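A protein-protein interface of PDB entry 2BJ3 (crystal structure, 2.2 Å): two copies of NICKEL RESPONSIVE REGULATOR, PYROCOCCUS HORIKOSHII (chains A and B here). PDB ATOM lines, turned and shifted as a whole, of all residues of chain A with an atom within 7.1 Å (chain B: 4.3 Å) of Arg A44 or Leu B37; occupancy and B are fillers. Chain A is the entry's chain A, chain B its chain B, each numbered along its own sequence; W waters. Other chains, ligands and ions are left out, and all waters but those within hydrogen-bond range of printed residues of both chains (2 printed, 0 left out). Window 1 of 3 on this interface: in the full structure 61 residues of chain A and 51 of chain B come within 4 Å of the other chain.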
ATOM      1  N   LEU A  14      20.508  -6.081 -13.623  1.00  0.00           N
ATOM      2  CA  LEU A  14      20.998  -4.759 -13.949  1.00  0.00           C
ATOM      3  C   LEU A  14      21.099  -3.938 -12.674  1.00  0.00           C
ATOM      4  O   LEU A  14      22.127  -3.322 -12.398  1.00  0.00           O
ATOM      5  CB  LEU A  14      20.038  -4.096 -14.935  1.00  0.00           C
ATOM      6  CG  LEU A  14      20.593  -3.025 -15.866  1.00  0.00           C
ATOM      7  CD1 LEU A  14      21.711  -3.622 -16.708  1.00  0.00           C
ATOM      8  CD2 LEU A  14      19.476  -2.494 -16.755  1.00  0.00           C
ATOM      9  N   PHE A  18      24.229  -2.323 -10.763  1.00  0.00           N
ATOM     10  CA  PHE A  18      24.149  -0.871 -10.659  1.00  0.00           C
ATOM     11  C   PHE A  18      24.404  -0.474  -9.213  1.00  0.00           C
ATOM     12  O   PHE A  18      25.182   0.446  -8.950  1.00  0.00           O
ATOM     13  CB  PHE A  18      22.766  -0.373 -11.093  1.00  0.00           C
ATOM     14  CG  PHE A  18      22.631   1.126 -11.096  1.00  0.00           C
ATOM     15  CD1 PHE A  18      23.225   1.890 -12.092  1.00  0.00           C
ATOM     16  CD2 PHE A  18      21.909   1.774 -10.099  1.00  0.00           C
ATOM     17  CE1 PHE A  18      23.103   3.293 -12.098  1.00  0.00           C
ATOM     18  CE2 PHE A  18      21.781   3.176 -10.094  1.00  0.00           C
ATOM     19  CZ  PHE A  18      22.380   3.931 -11.100  1.00  0.00           C
ATOM     20  N   ILE A  34      20.888   8.201 -10.228  1.00  0.00           N
ATOM     21  CA  ILE A  34      19.986   8.266 -11.366  1.00  0.00           C
ATOM     22  C   ILE A  34      19.794   9.701 -11.822  1.00  0.00           C
ATOM     23  O   ILE A  34      19.654   9.955 -13.017  1.00  0.00           O
ATOM     24  CB  ILE A  34      18.653   7.589 -11.024  1.00  0.00           C
ATOM     25  CG1 ILE A  34      18.883   6.077 -10.954  1.00  0.00           C
ATOM     26  CG2 ILE A  34      17.579   7.934 -12.065  1.00  0.00           C
ATOM     27  CD1 ILE A  34      17.689   5.276 -10.441  1.00  0.00           C
ATOM     28  N   ASP A  36      22.001  12.021 -11.795  1.00  0.00           N
ATOM     29  CA  ASP A  36      23.177  12.288 -12.615  1.00  0.00           C
ATOM     30  C   ASP A  36      23.052  11.682 -13.987  1.00  0.00           C
ATOM     31  O   ASP A  36      23.437  12.299 -14.977  1.00  0.00           O
ATOM     32  CB  ASP A  36      24.439  11.759 -11.931  1.00  0.00           C
ATOM     33  CG  ASP A  36      24.837  12.589 -10.735  1.00  0.00           C
ATOM     34  OD1 ASP A  36      24.016  13.424 -10.309  1.00  0.00           O
ATOM     35  OD2 ASP A  36      25.959  12.408 -10.218  1.00  0.00           O
ATOM     36  N   LEU A  37      22.523  10.459 -14.050  1.00  0.00           N
ATOM     37  CA  LEU A  37      22.350   9.790 -15.330  1.00  0.00           C
ATOM     38  C   LEU A  37      21.324  10.546 -16.170  1.00  0.00           C
ATOM     39  O   LEU A  37      21.482  10.673 -17.378  1.00  0.00           O
ATOM     40  CB  LEU A  37      21.876   8.352 -15.130  1.00  0.00           C
ATOM     41  CG  LEU A  37      22.841   7.303 -14.585  1.00  0.00           C
ATOM     42  CD1 LEU A  37      22.087   5.985 -14.433  1.00  0.00           C
ATOM     43  CD2 LEU A  37      24.007   7.130 -15.549  1.00  0.00           C
ATOM     44  N   ILE A  38      20.263  11.034 -15.526  1.00  0.00           N
ATOM     45  CA  ILE A  38      19.235  11.793 -16.233  1.00  0.00           C
ATOM     46  C   ILE A  38      19.782  13.147 -16.698  1.00  0.00           C
ATOM     47  O   ILE A  38      19.405  13.622 -17.765  1.00  0.00           O
ATOM     48  CB  ILE A  38      17.960  11.987 -15.346  1.00  0.00           C
ATOM     49  CG1 ILE A  38      17.187  10.662 -15.253  1.00  0.00           C
ATOM     50  CG2 ILE A  38      17.040  13.052 -15.937  1.00  0.00           C
ATOM     51  CD1 ILE A  38      16.069  10.668 -14.223  1.00  0.00           C
ATOM     52  N   ARG A  39      20.689  13.749 -15.926  1.00  0.00           N
ATOM     53  CA  ARG A  39      21.264  15.037 -16.315  1.00  0.00           C
ATOM     54  C   ARG A  39      22.117  14.925 -17.571  1.00  0.00           C
ATOM     55  O   ARG A  39      22.020  15.760 -18.474  1.00  0.00           O
ATOM     56  CB  ARG A  39      22.139  15.631 -15.211  1.00  0.00           C
ATOM     57  CG  ARG A  39      21.429  16.083 -13.963  1.00  0.00           C
ATOM     58  CD  ARG A  39      22.417  16.809 -13.042  1.00  0.00           C
ATOM     59  NE  ARG A  39      21.821  17.138 -11.752  1.00  0.00           N
ATOM     60  CZ  ARG A  39      21.579  16.254 -10.792  1.00  0.00           C
ATOM     61  NH1 ARG A  39      21.892  14.982 -10.979  1.00  0.00           N
ATOM     62  NH2 ARG A  39      21.019  16.635  -9.651  1.00  0.00           N
ATOM     63  N   ASP A  40      22.974  13.909 -17.632  1.00  0.00           N
ATOM     64  CA  ASP A  40      23.816  13.749 -18.806  1.00  0.00           C
ATOM     65  C   ASP A  40      22.964  13.394 -20.025  1.00  0.00           C
ATOM     66  O   ASP A  40      23.259  13.794 -21.151  1.00  0.00           O
ATOM     67  CB  ASP A  40      24.877  12.668 -18.579  1.00  0.00           C
ATOM     68  CG  ASP A  40      25.579  12.258 -19.879  1.00  0.00           C
ATOM     69  OD1 ASP A  40      26.161  13.138 -20.555  1.00  0.00           O
ATOM     70  OD2 ASP A  40      25.545  11.057 -20.233  1.00  0.00           O
ATOM     71  N   PHE A  41      21.910  12.631 -19.796  1.00  0.00           N
ATOM     72  CA  PHE A  41      21.025  12.228 -20.883  1.00  0.00           C
ATOM     73  C   PHE A  41      20.369  13.454 -21.546  1.00  0.00           C
ATOM     74  O   PHE A  41      20.263  13.537 -22.761  1.00  0.00           O
ATOM     75  CB  PHE A  41      19.960  11.279 -20.325  1.00  0.00           C
ATOM     76  CG  PHE A  41      18.851  10.976 -21.282  1.00  0.00           C
ATOM     77  CD1 PHE A  41      19.062  10.164 -22.382  1.00  0.00           C
ATOM     78  CD2 PHE A  41      17.584  11.517 -21.081  1.00  0.00           C
ATOM     79  CE1 PHE A  41      18.023   9.893 -23.270  1.00  0.00           C
ATOM     80  CE2 PHE A  41      16.545  11.253 -21.960  1.00  0.00           C
ATOM     81  CZ  PHE A  41      16.764  10.444 -23.053  1.00  0.00           C
ATOM     82  N   ILE A  42      19.927  14.409 -20.737  1.00  0.00           N
ATOM     83  CA  ILE A  42      19.284  15.615 -21.263  1.00  0.00           C
ATOM     84  C   ILE A  42      20.257  16.418 -22.122  1.00  0.00           C
ATOM     85  O   ILE A  42      19.903  16.917 -23.192  1.00  0.00           O
ATOM     86  CB  ILE A  42      18.784  16.507 -20.118  1.00  0.00           C
ATOM     87  CG1 ILE A  42      17.663  15.800 -19.366  1.00  0.00           C
ATOM     88  CG2 ILE A  42      18.293  17.827 -20.673  1.00  0.00           C
ATOM     89  CD1 ILE A  42      17.339  16.407 -18.023  1.00  0.00           C
ATOM     90  N   ILE A  43      21.488  16.534 -21.644  1.00  0.00           N
ATOM     91  CA  ILE A  43      22.512  17.265 -22.365  1.00  0.00           C
ATOM     92  C   ILE A  43      22.791  16.651 -23.726  1.00  0.00           C
ATOM     93  O   ILE A  43      22.960  17.370 -24.713  1.00  0.00           O
ATOM     94  CB  ILE A  43      23.816  17.310 -21.545  1.00  0.00           C
ATOM     95  CG1 ILE A  43      23.671  18.316 -20.407  1.00  0.00           C
ATOM     96  CG2 ILE A  43      24.986  17.683 -22.427  1.00  0.00           C
ATOM     97  CD1 ILE A  43      24.754  18.189 -19.342  1.00  0.00           C
ATOM     98  N   ARG A  44      22.834  15.323 -23.786  1.00  0.00           N
ATOM     99  CA  ARG A  44      23.110  14.631 -25.039  1.00  0.00           C
ATOM    100  C   ARG A  44      21.977  14.678 -26.050  1.00  0.00           C
ATOM    101  O   ARG A  44      22.213  14.574 -27.247  1.00  0.00           O
ATOM    102  CB  ARG A  44      23.480  13.174 -24.758  1.00  0.00           C
ATOM    103  CG  ARG A  44      24.849  13.021 -24.103  1.00  0.00           C
ATOM    104  CD  ARG A  44      25.225  11.561 -23.899  1.00  0.00           C
ATOM    105  NE  ARG A  44      24.441  10.944 -22.837  1.00  0.00           N
ATOM    106  CZ  ARG A  44      23.555   9.970 -23.019  1.00  0.00           C
ATOM    107  NH1 ARG A  44      23.337   9.489 -24.238  1.00  0.00           N
ATOM    108  NH2 ARG A  44      22.882   9.484 -21.980  1.00  0.00           N
ATOM    109  N   HIS A  45      20.747  14.849 -25.574  1.00  0.00           N
ATOM    110  CA  HIS A  45      19.585  14.894 -26.464  1.00  0.00           C
ATOM    111  C   HIS A  45      18.866  16.229 -26.587  1.00  0.00           C
ATOM    112  O   HIS A  45      17.884  16.322 -27.303  1.00  0.00           O
ATOM    113  CB  HIS A  45      18.570  13.832 -26.046  1.00  0.00           C
ATOM    114  CG  HIS A  45      19.032  12.436 -26.309  1.00  0.00           C
ATOM    115  ND1 HIS A  45      19.087  11.898 -27.578  1.00  0.00           N
ATOM    116  CD2 HIS A  45      19.511  11.484 -25.476  1.00  0.00           C
ATOM    117  CE1 HIS A  45      19.582  10.675 -27.513  1.00  0.00           C
ATOM    118  NE2 HIS A  45      19.848  10.400 -26.248  1.00  0.00           N
ATOM    119  N   GLU A  46      19.338  17.257 -25.895  1.00  0.00           N
ATOM    120  CA  GLU A  46      18.692  18.561 -25.986  1.00  0.00           C
ATOM    121  C   GLU A  46      18.473  18.997 -27.438  1.00  0.00           C
ATOM    122  O   GLU A  46      17.371  19.400 -27.807  1.00  0.00           O
ATOM    123  CB  GLU A  46      19.523  19.614 -25.254  1.00  0.00           C
ATOM    124  CG  GLU A  46      19.130  19.789 -23.803  1.00  0.00           C
ATOM    125  CD  GLU A  46      20.049  20.737 -23.059  1.00  0.00           C
ATOM    126  OE1 GLU A  46      19.760  21.052 -21.883  1.00  0.00           O
ATOM    127  OE2 GLU A  46      21.067  21.159 -23.651  1.00  0.00           O
ATOM    128  N   TRP A  47      19.520  18.899 -28.255  1.00  0.00           N
ATOM    129  CA  TRP A  47      19.477  19.288 -29.661  1.00  0.00           C
ATOM    130  C   TRP A  47      18.243  18.796 -30.445  1.00  0.00           C
ATOM    131  O   TRP A  47      17.943  19.299 -31.530  1.00  0.00           O
ATOM    132  CB  TRP A  47      20.736  18.782 -30.368  1.00  0.00           C
ATOM    133  CG  TRP A  47      20.720  17.292 -30.588  1.00  0.00           C
ATOM    134  CD1 TRP A  47      21.090  16.323 -29.700  1.00  0.00           C
ATOM    135  CD2 TRP A  47      20.299  16.610 -31.772  1.00  0.00           C
ATOM    136  NE1 TRP A  47      20.929  15.075 -30.260  1.00  0.00           N
ATOM    137  CE2 TRP A  47      20.445  15.223 -31.532  1.00  0.00           C
ATOM    138  CE3 TRP A  47      19.813  17.036 -33.016  1.00  0.00           C
ATOM    139  CZ2 TRP A  47      20.124  14.261 -32.490  1.00  0.00           C
ATOM    140  CZ3 TRP A  47      19.491  16.081 -33.970  1.00  0.00           C
ATOM    141  CH2 TRP A  47      19.649  14.707 -33.700  1.00  0.00           C
ATOM    142  N   GLU A  48      17.552  17.799 -29.913  1.00  0.00           N
ATOM    143  CA  GLU A  48      16.381  17.247 -30.582  1.00  0.00           C
ATOM    144  C   GLU A  48      15.118  18.013 -30.222  1.00  0.00           C
ATOM    145  O   GLU A  48      14.070  17.820 -30.833  1.00  0.00           O
ATOM    146  CB  GLU A  48      16.225  15.763 -30.230  1.00  0.00           C
ATOM    147  CG  GLU A  48      17.014  14.850 -31.148  1.00  0.00           C
ATOM    148  CD  GLU A  48      16.854  13.376 -30.827  1.00  0.00           C
ATOM    149  OE1 GLU A  48      17.424  12.913 -29.815  1.00  0.00           O
ATOM    150  OE2 GLU A  48      16.159  12.678 -31.592  1.00  0.00           O
ATOM    151  N   LYS A 127      25.179   6.079 -33.017  1.00  0.00           N
ATOM    152  CA  LYS A 127      25.136   6.995 -31.890  1.00  0.00           C
ATOM    153  C   LYS A 127      25.418   8.403 -32.375  1.00  0.00           C
ATOM    154  O   LYS A 127      26.251   8.612 -33.250  1.00  0.00           O
ATOM    155  CB  LYS A 127      26.143   6.603 -30.814  1.00  0.00           C
ATOM    156  CG  LYS A 127      25.485   6.422 -29.464  1.00  0.00           C
ATOM    157  CD  LYS A 127      26.476   6.433 -28.320  1.00  0.00           C
ATOM    158  CE  LYS A 127      25.742   6.474 -26.990  1.00  0.00           C
ATOM    159  NZ  LYS A 127      26.662   6.542 -25.826  1.00  0.00           N
ATOM    160  N   LEU A 128      24.719   9.368 -31.800  1.00  0.00           N
ATOM    161  CA  LEU A 128      24.893  10.749 -32.219  1.00  0.00           C
ATOM    162  C   LEU A 128      25.409  11.663 -31.129  1.00  0.00           C
ATOM    163  O   LEU A 128      25.032  11.554 -29.966  1.00  0.00           O
ATOM    164  CB  LEU A 128      23.572  11.315 -32.750  1.00  0.00           C
ATOM    165  CG  LEU A 128      23.020  10.740 -34.065  1.00  0.00           C
ATOM    166  CD1 LEU A 128      22.550   9.305 -33.868  1.00  0.00           C
ATOM    167  CD2 LEU A 128      21.859  11.591 -34.544  1.00  0.00           C
ATOM    168  N   VAL A 129      26.310  12.549 -31.516  1.00  0.00           N
ATOM    169  CA  VAL A 129      26.828  13.539 -30.592  1.00  0.00           C
ATOM    170  C   VAL A 129      26.480  14.817 -31.365  1.00  0.00           C
ATOM    171  O   VAL A 129      27.029  15.085 -32.429  1.00  0.00           O
ATOM    172  CB  VAL A 129      28.352  13.354 -30.375  1.00  0.00           C
ATOM    173  CG1 VAL A 129      28.899  14.449 -29.475  1.00  0.00           C
ATOM    174  CG2 VAL A 129      28.611  11.982 -29.712  1.00  0.00           C
ATOM    175  N   MET A 130      25.507  15.564 -30.858  1.00  0.00           N
ATOM    176  CA  MET A 130      25.055  16.766 -31.548  1.00  0.00           C
ATOM    177  C   MET A 130      24.872  17.918 -30.605  1.00  0.00           C
ATOM    178  O   MET A 130      24.627  17.713 -29.419  1.00  0.00           O
ATOM    179  CB  MET A 130      23.691  16.538 -32.209  1.00  0.00           C
ATOM    180  CG  MET A 130      23.642  15.548 -33.320  1.00  0.00           C
ATOM    181  SD  MET A 130      24.405  16.160 -34.764  1.00  0.00           S
ATOM    182  CE  MET A 130      24.822  14.624 -35.520  1.00  0.00           C
ATOM    183  N   THR A 131      24.956  19.127 -31.157  1.00  0.00           N
ATOM    184  CA  THR A 131      24.738  20.340 -30.383  1.00  0.00           C
ATOM    185  C   THR A 131      24.370  21.477 -31.327  1.00  0.00           C
ATOM    186  O   THR A 131      24.810  21.518 -32.473  1.00  0.00           O
ATOM    187  CB  THR A 131      25.983  20.732 -29.565  1.00  0.00           C
ATOM    188  OG1 THR A 131      25.593  21.657 -28.547  1.00  0.00           O
ATOM    189  CG2 THR A 131      27.028  21.383 -30.445  1.00  0.00           C
ATOM    190  N   ALA B  33      13.463   4.134 -20.235  1.00  0.00           N
ATOM    191  CA  ALA B  33      14.528   5.090 -20.539  1.00  0.00           C
ATOM    192  C   ALA B  33      15.675   4.963 -19.530  1.00  0.00           C
ATOM    193  O   ALA B  33      16.836   4.874 -19.902  1.00  0.00           O
ATOM    194  CB  ALA B  33      13.974   6.504 -20.510  1.00  0.00           C
ATOM    195  N   ILE B  34      15.333   4.960 -18.254  1.00  0.00           N
ATOM    196  CA  ILE B  34      16.320   4.851 -17.196  1.00  0.00           C
ATOM    197  C   ILE B  34      17.054   3.506 -17.269  1.00  0.00           C
ATOM    198  O   ILE B  34      18.238   3.430 -16.955  1.00  0.00           O
ATOM    199  CB  ILE B  34      15.640   5.036 -15.845  1.00  0.00           C
ATOM    200  CG1 ILE B  34      15.151   6.484 -15.739  1.00  0.00           C
ATOM    201  CG2 ILE B  34      16.578   4.669 -14.712  1.00  0.00           C
ATOM    202  CD1 ILE B  34      14.382   6.798 -14.466  1.00  0.00           C
ATOM    203  N   ARG B  35      16.346   2.458 -17.694  1.00  0.00           N
ATOM    204  CA  ARG B  35      16.930   1.133 -17.832  1.00  0.00           C
ATOM    205  C   ARG B  35      18.074   1.232 -18.851  1.00  0.00           C
ATOM    206  O   ARG B  35      19.162   0.706 -18.634  1.00  0.00           O
ATOM    207  CB  ARG B  35      15.869   0.150 -18.324  1.00  0.00           C
ATOM    208  CG  ARG B  35      16.318  -1.297 -18.364  1.00  0.00           C
ATOM    209  CD  ARG B  35      15.725  -2.002 -19.565  1.00  0.00           C
ATOM    210  NE  ARG B  35      14.264  -1.972 -19.571  1.00  0.00           N
ATOM    211  CZ  ARG B  35      13.528  -1.778 -20.664  1.00  0.00           C
ATOM    212  NH1 ARG B  35      14.119  -1.592 -21.838  1.00  0.00           N
ATOM    213  NH2 ARG B  35      12.203  -1.779 -20.590  1.00  0.00           N
ATOM    214  N   ASP B  36      17.821   1.916 -19.964  1.00  0.00           N
ATOM    215  CA  ASP B  36      18.840   2.102 -20.991  1.00  0.00           C
ATOM    216  C   ASP B  36      20.030   2.920 -20.480  1.00  0.00           C
ATOM    217  O   ASP B  36      21.167   2.648 -20.841  1.00  0.00           O
ATOM    218  CB  ASP B  36      18.258   2.808 -22.213  1.00  0.00           C
ATOM    219  CG  ASP B  36      17.442   1.886 -23.092  1.00  0.00           C
ATOM    220  OD1 ASP B  36      17.203   2.261 -24.261  1.00  0.00           O
ATOM    221  OD2 ASP B  36      17.034   0.799 -22.621  1.00  0.00           O
ATOM    222  N   LEU B  37      19.756   3.931 -19.656  1.00  0.00           N
ATOM    223  CA  LEU B  37      20.809   4.782 -19.102  1.00  0.00           C
ATOM    224  C   LEU B  37      21.682   3.987 -18.142  1.00  0.00           C
ATOM    225  O   LEU B  37      22.902   4.123 -18.145  1.00  0.00           O
ATOM    226  CB  LEU B  37      20.209   5.968 -18.349  1.00  0.00           C
ATOM    227  CG  LEU B  37      19.381   6.993 -19.127  1.00  0.00           C
ATOM    228  CD1 LEU B  37      19.012   8.107 -18.186  1.00  0.00           C
ATOM    229  CD2 LEU B  37      20.165   7.544 -20.298  1.00  0.00           C
ATOM    230  N   ILE B  38      21.043   3.170 -17.312  1.00  0.00           N
ATOM    231  CA  ILE B  38      21.753   2.342 -16.352  1.00  0.00           C
ATOM    232  C   ILE B  38      22.614   1.295 -17.057  1.00  0.00           C
ATOM    233  O   ILE B  38      23.771   1.094 -16.710  1.00  0.00           O
ATOM    234  CB  ILE B  38      20.766   1.662 -15.408  1.00  0.00           C
ATOM    235  CG1 ILE B  38      20.173   2.706 -14.470  1.00  0.00           C
ATOM    236  CG2 ILE B  38      21.459   0.573 -14.611  1.00  0.00           C
ATOM    237  CD1 ILE B  38      19.046   2.196 -13.616  1.00  0.00           C
ATOM    238  N   ARG B  39      22.042   0.652 -18.062  1.00  0.00           N
ATOM    239  CA  ARG B  39      22.744  -0.355 -18.833  1.00  0.00           C
ATOM    240  C   ARG B  39      23.954   0.243 -19.544  1.00  0.00           C
ATOM    241  O   ARG B  39      25.018  -0.369 -19.580  1.00  0.00           O
ATOM    242  CB  ARG B  39      21.796  -0.978 -19.856  1.00  0.00           C
ATOM    243  CG  ARG B  39      22.435  -2.057 -20.675  1.00  0.00           C
ATOM    244  CD  ARG B  39      21.435  -2.790 -21.554  1.00  0.00           C
ATOM    245  NE  ARG B  39      22.048  -3.995 -22.118  1.00  0.00           N
ATOM    246  CZ  ARG B  39      22.925  -4.008 -23.120  1.00  0.00           C
ATOM    247  NH1 ARG B  39      23.308  -2.877 -23.703  1.00  0.00           N
ATOM    248  NH2 ARG B  39      23.437  -5.160 -23.528  1.00  0.00           N
ATOM    249  N   ASP B  40      23.800   1.434 -20.116  1.00  0.00           N
ATOM    250  CA  ASP B  40      24.922   2.071 -20.804  1.00  0.00           C
ATOM    251  C   ASP B  40      26.014   2.469 -19.813  1.00  0.00           C
ATOM    252  O   ASP B  40      27.202   2.378 -20.110  1.00  0.00           O
ATOM    253  CB  ASP B  40      24.463   3.307 -21.567  1.00  0.00           C
ATOM    254  CG  ASP B  40      23.796   2.964 -22.878  1.00  0.00           C
ATOM    255  OD1 ASP B  40      23.838   1.777 -23.275  1.00  0.00           O
ATOM    256  OD2 ASP B  40      23.238   3.886 -23.518  1.00  0.00           O
ATOM    257  N   PHE B  41      25.594   2.916 -18.638  1.00  0.00           N
ATOM    258  CA  PHE B  41      26.508   3.314 -17.570  1.00  0.00           C
ATOM    259  C   PHE B  41      27.364   2.119 -17.125  1.00  0.00           C
ATOM    260  O   PHE B  41      28.576   2.228 -16.953  1.00  0.00           O
ATOM    261  CB  PHE B  41      25.689   3.828 -16.390  1.00  0.00           C
ATOM    262  CG  PHE B  41      26.499   4.178 -15.189  1.00  0.00           C
ATOM    263  CD1 PHE B  41      26.591   3.300 -14.123  1.00  0.00           C
ATOM    264  CD2 PHE B  41      27.155   5.403 -15.108  1.00  0.00           C
ATOM    265  CE1 PHE B  41      27.321   3.634 -12.988  1.00  0.00           C
ATOM    266  CE2 PHE B  41      27.888   5.747 -13.977  1.00  0.00           C
ATOM    267  CZ  PHE B  41      27.970   4.862 -12.917  1.00  0.00           C
ATOM    268  N   HIS B 125      30.370  21.241 -26.492  1.00  0.00           N
ATOM    269  CA  HIS B 125      29.794  19.917 -26.305  1.00  0.00           C
ATOM    270  C   HIS B 125      30.759  18.888 -26.880  1.00  0.00           C
ATOM    271  O   HIS B 125      31.505  19.182 -27.815  1.00  0.00           O
ATOM    272  CB  HIS B 125      28.470  19.889 -27.091  1.00  0.00           C
ATOM    273  CG  HIS B 125      27.662  18.645 -26.926  1.00  0.00           C
ATOM    274  ND1 HIS B 125      26.944  18.368 -25.783  1.00  0.00           N
ATOM    275  CD2 HIS B 125      27.410  17.627 -27.785  1.00  0.00           C
ATOM    276  CE1 HIS B 125      26.285  17.234 -25.946  1.00  0.00           C
ATOM    277  NE2 HIS B 125      26.551  16.765 -27.151  1.00  0.00           N
ATOM    278  N   LYS B 127      31.802  14.227 -26.909  1.00  0.00           N
ATOM    279  CA  LYS B 127      31.639  12.929 -26.275  1.00  0.00           C
ATOM    280  C   LYS B 127      32.528  11.843 -26.851  1.00  0.00           C
ATOM    281  O   LYS B 127      32.903  11.861 -28.032  1.00  0.00           O
ATOM    282  CB  LYS B 127      30.182  12.474 -26.346  1.00  0.00           C
ATOM    283  CG  LYS B 127      29.854  11.340 -25.394  1.00  0.00           C
ATOM    284  CD  LYS B 127      28.408  10.877 -25.540  1.00  0.00           C
ATOM    285  CE  LYS B 127      28.090   9.737 -24.571  1.00  0.00           C
ATOM    286  NZ  LYS B 127      29.014   8.576 -24.752  1.00  0.00           N
HETATM  287  O   HOH W   1      24.555  15.005 -28.316  1.00  0.00           O
HETATM  288  O   HOH W   2      23.124   6.664 -22.045  1.00  0.00           O
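NZ of Lys B127 sits close to NZ of Lys A127, 3.3 Å away. The backbone carbonyl oxygen (O) of Met A130 sits at hydrogen-bond distance from a ring nitrogen (NE2) of His B125 (3.1 Å).
The guanidinium group of Arg B35 is in salt-bridge range of the side-chain carboxylate of Asp B36. The backbone carbonyl oxygen of Arg A44 sits close to the indole nitrogen of Trp A47 (3.3 Å). The guanidinium group of Arg A44 lies within salt-bridge range of the side-chain carboxylate of Asp A40, at 2.8 Å.
CG2 of Ile B38 touches CG of Leu A14, at 3.9 Å. O of Leu A37 touches CD1 of Leu B37, 3.7 Å away. Ile B38 touches Leu A37 (CG1 to CD1, 3.8 Å). Phe B41 touches Leu A37 (CD2 to CD2, 3.6 Å). CD2 of Leu B37 touches CD1 of Phe A41 (3.5 Å). Ile A43 touches His B125. Leu B37 touches Arg A44. His B125 touches Val A129. Val A129 touches Lys B127. CB of Thr A131 touches CB of His B125, at 3.6 Å.
Printed residues of chain B within 4 Å of Leu A37: Leu B37, Ile B38 and Phe B41. Of the printed residues of chain B, Ile A43 touches His B125. Arg A44 touches just these residues of chain B: Leu B37 (3.7 Å) and Lys B127 (3.5 Å). Of the printed residues of chain B, Thr A131 touches His B125 (3.6 Å). Leu B37 touches three residues of chain A. Of the printed residues of chain A, Phe B41 touches Leu A37 (3.6 Å). The nearest residue of chain B that does not touch Arg A44 is His B125 (4.2 Å). The nearest residue of chain A that does not touch Leu B37 is Ile A38 (4.1 Å).
Of the 11 printed residues of chain B, 6 touch a printed residue of chain A. Hydrophobic or aromatic side chains of chain B within 4 Å of the printed part of chain A: Leu B37, Ile B38, Phe B41 and His B125. Among the printed residues, 15 pairs touch across the chains. Among the printed residues, no Asp or Glu carboxylate lies within 4 Å of a Lys or Arg side-chain nitrogen of the other chain.
Leu B37 touches its own counterpart, Leu A37. Leu A37 touches Ile B38, but with the chains exchanged Ile A38 does not touch Leu B37 (4.1 Å). Leu A37 touches Phe B41, and with the chains exchanged Phe A41 touches Leu B37. Lys A127 touches its own counterpart, Lys B127.
Water W1 lies within hydrogen-bond range of O of Arg A44 (2.6 Å), N of Met A130 (2.8 Å) and NE2 of His B125 (2.9 Å). Water W2 lies within hydrogen-bond range of the guanidinium group of Arg A44 and the side-chain carboxylate of Asp B40.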
